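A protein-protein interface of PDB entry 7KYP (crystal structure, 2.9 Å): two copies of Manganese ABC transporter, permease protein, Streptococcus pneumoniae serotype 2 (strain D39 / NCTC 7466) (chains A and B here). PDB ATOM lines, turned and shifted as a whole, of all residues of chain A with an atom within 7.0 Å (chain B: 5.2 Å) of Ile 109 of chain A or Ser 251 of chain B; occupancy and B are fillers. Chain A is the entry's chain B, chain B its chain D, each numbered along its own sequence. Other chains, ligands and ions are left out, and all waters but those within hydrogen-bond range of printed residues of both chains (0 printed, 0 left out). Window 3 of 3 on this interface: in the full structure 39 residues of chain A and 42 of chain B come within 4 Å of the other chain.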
ATOM      1  N   ALA A  57      16.606 -27.699  -1.653  1.00  0.00           N
ATOM      2  CA  ALA A  57      17.863 -26.967  -1.805  1.00  0.00           C
ATOM      3  C   ALA A  57      17.899 -25.712  -0.934  1.00  0.00           C
ATOM      4  O   ALA A  57      18.910 -25.428  -0.290  1.00  0.00           O
ATOM      5  CB  ALA A  57      18.081 -26.597  -3.263  1.00  0.00           C
ATOM      6  N   LEU A 104      12.197 -26.721 -11.304  1.00  0.00           N
ATOM      7  CA  LEU A 104      13.334 -27.618 -11.521  1.00  0.00           C
ATOM      8  C   LEU A 104      14.609 -26.833 -11.827  1.00  0.00           C
ATOM      9  O   LEU A 104      15.666 -27.110 -11.258  1.00  0.00           O
ATOM     10  CB  LEU A 104      13.039 -28.594 -12.665  1.00  0.00           C
ATOM     11  CG  LEU A 104      14.184 -29.519 -13.099  1.00  0.00           C
ATOM     12  CD1 LEU A 104      14.624 -30.417 -11.953  1.00  0.00           C
ATOM     13  CD2 LEU A 104      13.776 -30.350 -14.302  1.00  0.00           C
ATOM     14  N   ALA A 105      14.500 -25.864 -12.732  1.00  0.00           N
ATOM     15  CA  ALA A 105      15.633 -25.019 -13.110  1.00  0.00           C
ATOM     16  C   ALA A 105      16.125 -24.180 -11.932  1.00  0.00           C
ATOM     17  O   ALA A 105      17.331 -24.017 -11.742  1.00  0.00           O
ATOM     18  CB  ALA A 105      15.256 -24.119 -14.277  1.00  0.00           C
ATOM     19  N   LEU A 106      15.188 -23.649 -11.149  1.00  0.00           N
ATOM     20  CA  LEU A 106      15.520 -22.897  -9.938  1.00  0.00           C
ATOM     21  C   LEU A 106      16.293 -23.766  -8.946  1.00  0.00           C
ATOM     22  O   LEU A 106      17.266 -23.310  -8.345  1.00  0.00           O
ATOM     23  CB  LEU A 106      14.247 -22.357  -9.276  1.00  0.00           C
ATOM     24  CG  LEU A 106      14.408 -21.549  -7.983  1.00  0.00           C
ATOM     25  CD1 LEU A 106      15.275 -20.320  -8.209  1.00  0.00           C
ATOM     26  CD2 LEU A 106      13.045 -21.152  -7.436  1.00  0.00           C
ATOM     27  N   GLY A 107      15.853 -25.012  -8.785  1.00  0.00           N
ATOM     28  CA  GLY A 107      16.504 -25.963  -7.885  1.00  0.00           C
ATOM     29  C   GLY A 107      17.949 -26.261  -8.245  1.00  0.00           C
ATOM     30  O   GLY A 107      18.796 -26.386  -7.362  1.00  0.00           O
ATOM     31  N   ILE A 108      18.230 -26.371  -9.542  1.00  0.00           N
ATOM     32  CA  ILE A 108      19.593 -26.627 -10.025  1.00  0.00           C
ATOM     33  C   ILE A 108      20.515 -25.437  -9.732  1.00  0.00           C
ATOM     34  O   ILE A 108      21.689 -25.625  -9.402  1.00  0.00           O
ATOM     35  CB  ILE A 108      19.608 -26.961 -11.538  1.00  0.00           C
ATOM     36  CG1 ILE A 108      18.901 -28.298 -11.792  1.00  0.00           C
ATOM     37  CG2 ILE A 108      21.037 -27.026 -12.071  1.00  0.00           C
ATOM     38  CD1 ILE A 108      18.602 -28.577 -13.250  1.00  0.00           C
ATOM     39  N   ILE A 109      19.980 -24.222  -9.846  1.00  0.00           N
ATOM     40  CA  ILE A 109      20.743 -23.005  -9.561  1.00  0.00           C
ATOM     41  C   ILE A 109      21.071 -22.901  -8.069  1.00  0.00           C
ATOM     42  O   ILE A 109      22.210 -22.607  -7.701  1.00  0.00           O
ATOM     43  CB  ILE A 109      19.983 -21.734 -10.019  1.00  0.00           C
ATOM     44  CG1 ILE A 109      19.818 -21.714 -11.547  1.00  0.00           C
ATOM     45  CG2 ILE A 109      20.692 -20.467  -9.550  1.00  0.00           C
ATOM     46  CD1 ILE A 109      21.085 -21.415 -12.324  1.00  0.00           C
ATOM     47  N   LEU A 110      20.074 -23.145  -7.219  1.00  0.00           N
ATOM     48  CA  LEU A 110      20.251 -23.065  -5.764  1.00  0.00           C
ATOM     49  C   LEU A 110      21.212 -24.128  -5.221  1.00  0.00           C
ATOM     50  O   LEU A 110      21.923 -23.883  -4.244  1.00  0.00           O
ATOM     51  CB  LEU A 110      18.898 -23.173  -5.050  1.00  0.00           C
ATOM     52  CG  LEU A 110      17.907 -22.027  -5.284  1.00  0.00           C
ATOM     53  CD1 LEU A 110      16.534 -22.387  -4.736  1.00  0.00           C
ATOM     54  CD2 LEU A 110      18.409 -20.729  -4.666  1.00  0.00           C
ATOM     55  N   ILE A 111      21.226 -25.303  -5.846  1.00  0.00           N
ATOM     56  CA  ILE A 111      22.157 -26.372  -5.476  1.00  0.00           C
ATOM     57  C   ILE A 111      23.578 -26.052  -5.949  1.00  0.00           C
ATOM     58  O   ILE A 111      24.546 -26.322  -5.236  1.00  0.00           O
ATOM     59  CB  ILE A 111      21.703 -27.736  -6.046  1.00  0.00           C
ATOM     60  CG1 ILE A 111      20.418 -28.190  -5.350  1.00  0.00           C
ATOM     61  CG2 ILE A 111      22.786 -28.797  -5.867  1.00  0.00           C
ATOM     62  CD1 ILE A 111      19.639 -29.243  -6.108  1.00  0.00           C
ATOM     63  N   GLY A 112      23.695 -25.480  -7.146  1.00  0.00           N
ATOM     64  CA  GLY A 112      24.994 -25.150  -7.729  1.00  0.00           C
ATOM     65  C   GLY A 112      25.783 -24.116  -6.945  1.00  0.00           C
ATOM     66  O   GLY A 112      26.995 -24.259  -6.768  1.00  0.00           O
ATOM     67  N   VAL A 113      25.100 -23.071  -6.481  1.00  0.00           N
ATOM     68  CA  VAL A 113      25.752 -22.001  -5.712  1.00  0.00           C
ATOM     69  C   VAL A 113      26.261 -22.470  -4.344  1.00  0.00           C
ATOM     70  O   VAL A 113      27.301 -22.005  -3.876  1.00  0.00           O
ATOM     71  CB  VAL A 113      24.840 -20.757  -5.524  1.00  0.00           C
ATOM     72  CG1 VAL A 113      24.538 -20.108  -6.868  1.00  0.00           C
ATOM     73  CG2 VAL A 113      23.551 -21.096  -4.778  1.00  0.00           C
ATOM     74  N   ALA A 114      25.531 -23.391  -3.715  1.00  0.00           N
ATOM     75  CA  ALA A 114      25.877 -23.882  -2.381  1.00  0.00           C
ATOM     76  C   ALA A 114      26.747 -25.135  -2.443  1.00  0.00           C
ATOM     77  O   ALA A 114      27.877 -25.135  -1.953  1.00  0.00           O
ATOM     78  CB  ALA A 114      24.612 -24.162  -1.584  1.00  0.00           C
ATOM     79  N   LEU A 120      24.614 -32.351  -6.848  1.00  0.00           N
ATOM     80  CA  LEU A 120      23.509 -32.130  -7.785  1.00  0.00           C
ATOM     81  C   LEU A 120      23.165 -33.412  -8.536  1.00  0.00           C
ATOM     82  O   LEU A 120      21.993 -33.759  -8.677  1.00  0.00           O
ATOM     83  CB  LEU A 120      23.863 -31.027  -8.787  1.00  0.00           C
ATOM     84  CG  LEU A 120      22.768 -30.627  -9.785  1.00  0.00           C
ATOM     85  CD1 LEU A 120      21.682 -29.809  -9.103  1.00  0.00           C
ATOM     86  CD2 LEU A 120      23.361 -29.851 -10.950  1.00  0.00           C
ATOM     87  N   ALA B 233      15.432 -14.948 -24.403  1.00  0.00           N
ATOM     88  CA  ALA B 233      15.658 -15.690 -23.159  1.00  0.00           C
ATOM     89  C   ALA B 233      16.935 -16.527 -23.224  1.00  0.00           C
ATOM     90  O   ALA B 233      17.629 -16.692 -22.219  1.00  0.00           O
ATOM     91  CB  ALA B 233      14.462 -16.579 -22.846  1.00  0.00           C
ATOM     92  N   GLY B 237      19.884 -15.621 -20.737  1.00  0.00           N
ATOM     93  CA  GLY B 237      20.217 -16.781 -19.919  1.00  0.00           C
ATOM     94  C   GLY B 237      21.693 -17.126 -19.983  1.00  0.00           C
ATOM     95  O   GLY B 237      22.307 -17.444 -18.963  1.00  0.00           O
ATOM     96  N   ILE B 240      23.618 -14.543 -18.012  1.00  0.00           N
ATOM     97  CA  ILE B 240      23.539 -14.813 -16.573  1.00  0.00           C
ATOM     98  C   ILE B 240      24.504 -15.935 -16.183  1.00  0.00           C
ATOM     99  O   ILE B 240      25.266 -15.800 -15.226  1.00  0.00           O
ATOM    100  CB  ILE B 240      22.100 -15.189 -16.138  1.00  0.00           C
ATOM    101  CG1 ILE B 240      21.150 -13.993 -16.302  1.00  0.00           C
ATOM    102  CG2 ILE B 240      22.072 -15.694 -14.697  1.00  0.00           C
ATOM    103  CD1 ILE B 240      21.271 -12.928 -15.232  1.00  0.00           C
ATOM    104  N   GLY B 241      24.461 -17.037 -16.929  1.00  0.00           N
ATOM    105  CA  GLY B 241      25.328 -18.187 -16.673  1.00  0.00           C
ATOM    106  C   GLY B 241      26.804 -17.880 -16.840  1.00  0.00           C
ATOM    107  O   GLY B 241      27.637 -18.382 -16.084  1.00  0.00           O
ATOM    108  N   VAL B 246      27.118 -19.910 -13.448  1.00  0.00           N
ATOM    109  CA  VAL B 246      26.046 -20.827 -13.054  1.00  0.00           C
ATOM    110  C   VAL B 246      25.464 -21.525 -14.281  1.00  0.00           C
ATOM    111  O   VAL B 246      25.735 -21.128 -15.417  1.00  0.00           O
ATOM    112  CB  VAL B 246      24.922 -20.104 -12.273  1.00  0.00           C
ATOM    113  CG1 VAL B 246      25.438 -19.635 -10.920  1.00  0.00           C
ATOM    114  CG2 VAL B 246      24.353 -18.932 -13.067  1.00  0.00           C
ATOM    115  N   ALA B 247      24.671 -22.568 -14.038  1.00  0.00           N
ATOM    116  CA  ALA B 247      24.073 -23.366 -15.109  1.00  0.00           C
ATOM    117  C   ALA B 247      23.299 -22.488 -16.092  1.00  0.00           C
ATOM    118  O   ALA B 247      22.260 -21.924 -15.747  1.00  0.00           O
ATOM    119  CB  ALA B 247      23.158 -24.431 -14.523  1.00  0.00           C
ATOM    120  N   ALA B 248      23.819 -22.377 -17.313  1.00  0.00           N
ATOM    121  CA  ALA B 248      23.226 -21.514 -18.335  1.00  0.00           C
ATOM    122  C   ALA B 248      21.872 -22.037 -18.807  1.00  0.00           C
ATOM    123  O   ALA B 248      20.936 -21.260 -18.988  1.00  0.00           O
ATOM    124  CB  ALA B 248      24.173 -21.359 -19.514  1.00  0.00           C
ATOM    125  N   GLY B 249      21.772 -23.350 -19.001  1.00  0.00           N
ATOM    126  CA  GLY B 249      20.512 -23.981 -19.393  1.00  0.00           C
ATOM    127  C   GLY B 249      19.359 -23.619 -18.471  1.00  0.00           C
ATOM    128  O   GLY B 249      18.266 -23.295 -18.935  1.00  0.00           O
ATOM    129  N   SER B 250      19.611 -23.672 -17.164  1.00  0.00           N
ATOM    130  CA  SER B 250      18.614 -23.292 -16.161  1.00  0.00           C
ATOM    131  C   SER B 250      18.359 -21.783 -16.153  1.00  0.00           C
ATOM    132  O   SER B 250      17.226 -21.343 -15.955  1.00  0.00           O
ATOM    133  CB  SER B 250      19.054 -23.749 -14.769  1.00  0.00           C
ATOM    134  OG  SER B 250      19.174 -25.159 -14.714  1.00  0.00           O
ATOM    135  N   SER B 251      19.417 -20.999 -16.358  1.00  0.00           N
ATOM    136  CA  SER B 251      19.306 -19.541 -16.439  1.00  0.00           C
ATOM    137  C   SER B 251      18.473 -19.097 -17.644  1.00  0.00           C
ATOM    138  O   SER B 251      17.762 -18.093 -17.575  1.00  0.00           O
ATOM    139  CB  SER B 251      20.696 -18.905 -16.513  1.00  0.00           C
ATOM    140  OG  SER B 251      21.505 -19.311 -15.421  1.00  0.00           O
ATOM    141  N   ILE B 252      18.574 -19.843 -18.741  1.00  0.00           N
ATOM    142  CA  ILE B 252      17.761 -19.599 -19.934  1.00  0.00           C
ATOM    143  C   ILE B 252      16.279 -19.879 -19.659  1.00  0.00           C
ATOM    144  O   ILE B 252      15.409 -19.131 -20.110  1.00  0.00           O
ATOM    145  CB  ILE B 252      18.258 -20.449 -21.130  1.00  0.00           C
ATOM    146  CG1 ILE B 252      19.619 -19.935 -21.615  1.00  0.00           C
ATOM    147  CG2 ILE B 252      17.254 -20.427 -22.277  1.00  0.00           C
ATOM    148  CD1 ILE B 252      20.324 -20.858 -22.588  1.00  0.00           C
ATOM    149  N   VAL B 253      16.002 -20.949 -18.917  1.00  0.00           N
ATOM    150  CA  VAL B 253      14.626 -21.326 -18.575  1.00  0.00           C
ATOM    151  C   VAL B 253      13.993 -20.326 -17.606  1.00  0.00           C
ATOM    152  O   VAL B 253      12.832 -19.948 -17.776  1.00  0.00           O
ATOM    153  CB  VAL B 253      14.560 -22.755 -17.988  1.00  0.00           C
ATOM    154  CG1 VAL B 253      13.175 -23.058 -17.429  1.00  0.00           C
ATOM    155  CG2 VAL B 253      14.932 -23.778 -19.052  1.00  0.00           C
ATOM    156  N   LEU B 254      14.752 -19.902 -16.598  1.00  0.00           N
ATOM    157  CA  LEU B 254      14.267 -18.918 -15.627  1.00  0.00           C
ATOM    158  C   LEU B 254      14.003 -17.558 -16.272  1.00  0.00           C
ATOM    159  O   LEU B 254      13.075 -16.853 -15.876  1.00  0.00           O
ATOM    160  CB  LEU B 254      15.257 -18.760 -14.468  1.00  0.00           C
ATOM    161  CG  LEU B 254      15.371 -19.947 -13.508  1.00  0.00           C
ATOM    162  CD1 LEU B 254      16.551 -19.756 -12.568  1.00  0.00           C
ATOM    163  CD2 LEU B 254      14.083 -20.147 -12.721  1.00  0.00           C
ATOM    164  N   THR B 255      14.821 -17.194 -17.257  1.00  0.00           N
ATOM    165  CA  THR B 255      14.622 -15.955 -18.009  1.00  0.00           C
ATOM    166  C   THR B 255      13.337 -16.020 -18.834  1.00  0.00           C
ATOM    167  O   THR B 255      12.600 -15.037 -18.923  1.00  0.00           O
ATOM    168  CB  THR B 255      15.812 -15.660 -18.944  1.00  0.00           C
ATOM    169  OG1 THR B 255      17.032 -15.671 -18.192  1.00  0.00           O
ATOM    170  CG2 THR B 255      15.649 -14.303 -19.617  1.00  0.00           C
ATOM    171  N   ALA B 256      13.079 -17.176 -19.439  1.00  0.00           N
ATOM    172  CA  ALA B 256      11.839 -17.403 -20.181  1.00  0.00           C
ATOM    173  C   ALA B 256      10.632 -17.397 -19.245  1.00  0.00           C
ATOM    174  O   ALA B 256       9.572 -16.880 -19.596  1.00  0.00           O
ATOM    175  CB  ALA B 256      11.910 -18.718 -20.943  1.00  0.00           C
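The backbone carbonyl oxygen (O) of Ala 247 of chain B sits at hydrogen-bond distance from the side-chain hydroxyl (OG) of Ser 251 of chain B (2.7 Å). O of Ser 251 of chain B sits at hydrogen-bond distance from OG1 of Thr 255 of chain B (2.6 Å).
Printed residues of chain B within 4 Å of Leu 106 of chain A: Leu 254. Of the printed residues of chain A, Leu 254 of chain B touches Leu 106 and Ile 109. Of the printed residues of chain A, Ser 250 of chain B touches Ala 105, Ile 108 and Ile 109. Of the printed residues of chain B, Ala 105 of chain A touches Ser 250 and Val 253. Leu 110 of chain A touches none of the printed residues of chain B. The nearest residue of chain B that does not touch Ile 109 of chain A is Val 246 of chain B (4.1 Å).
No position is printed for both chains.
Among the printed residues, pairs that only touch across the chains: Ala 105 of chain A with Ser 250 of chain B (3.5 Å), Ile 109 of chain A with Ala 247 of chain B (3.7 Å), Ile 108 of chain A with Ser 250 of chain B (3.7 Å), Ile 109 of chain A with Ser 251 of chain B (3.8 Å), Ile 109 of chain A with Ser 250 of chain B (3.9 Å), Ala 105 of chain A with Val 253 of chain B (3.9 Å), Ile 109 of chain A with Leu 254 of chain B (3.9 Å) and Leu 106 of chain A with Leu 254 of chain B (3.99 Å).
Hydrophobic or aromatic side chains of chain B that line the printed part of chain A: Val 253 and Leu 254. Printed residues of chain A that touch a printed residue of chain B: Ala 105, Leu 106, Ile 108 and Ile 109. Among the printed residues, no Asp or Glu carboxylate lies within 4 Å of a Lys or Arg side-chain nitrogen of the other chain.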
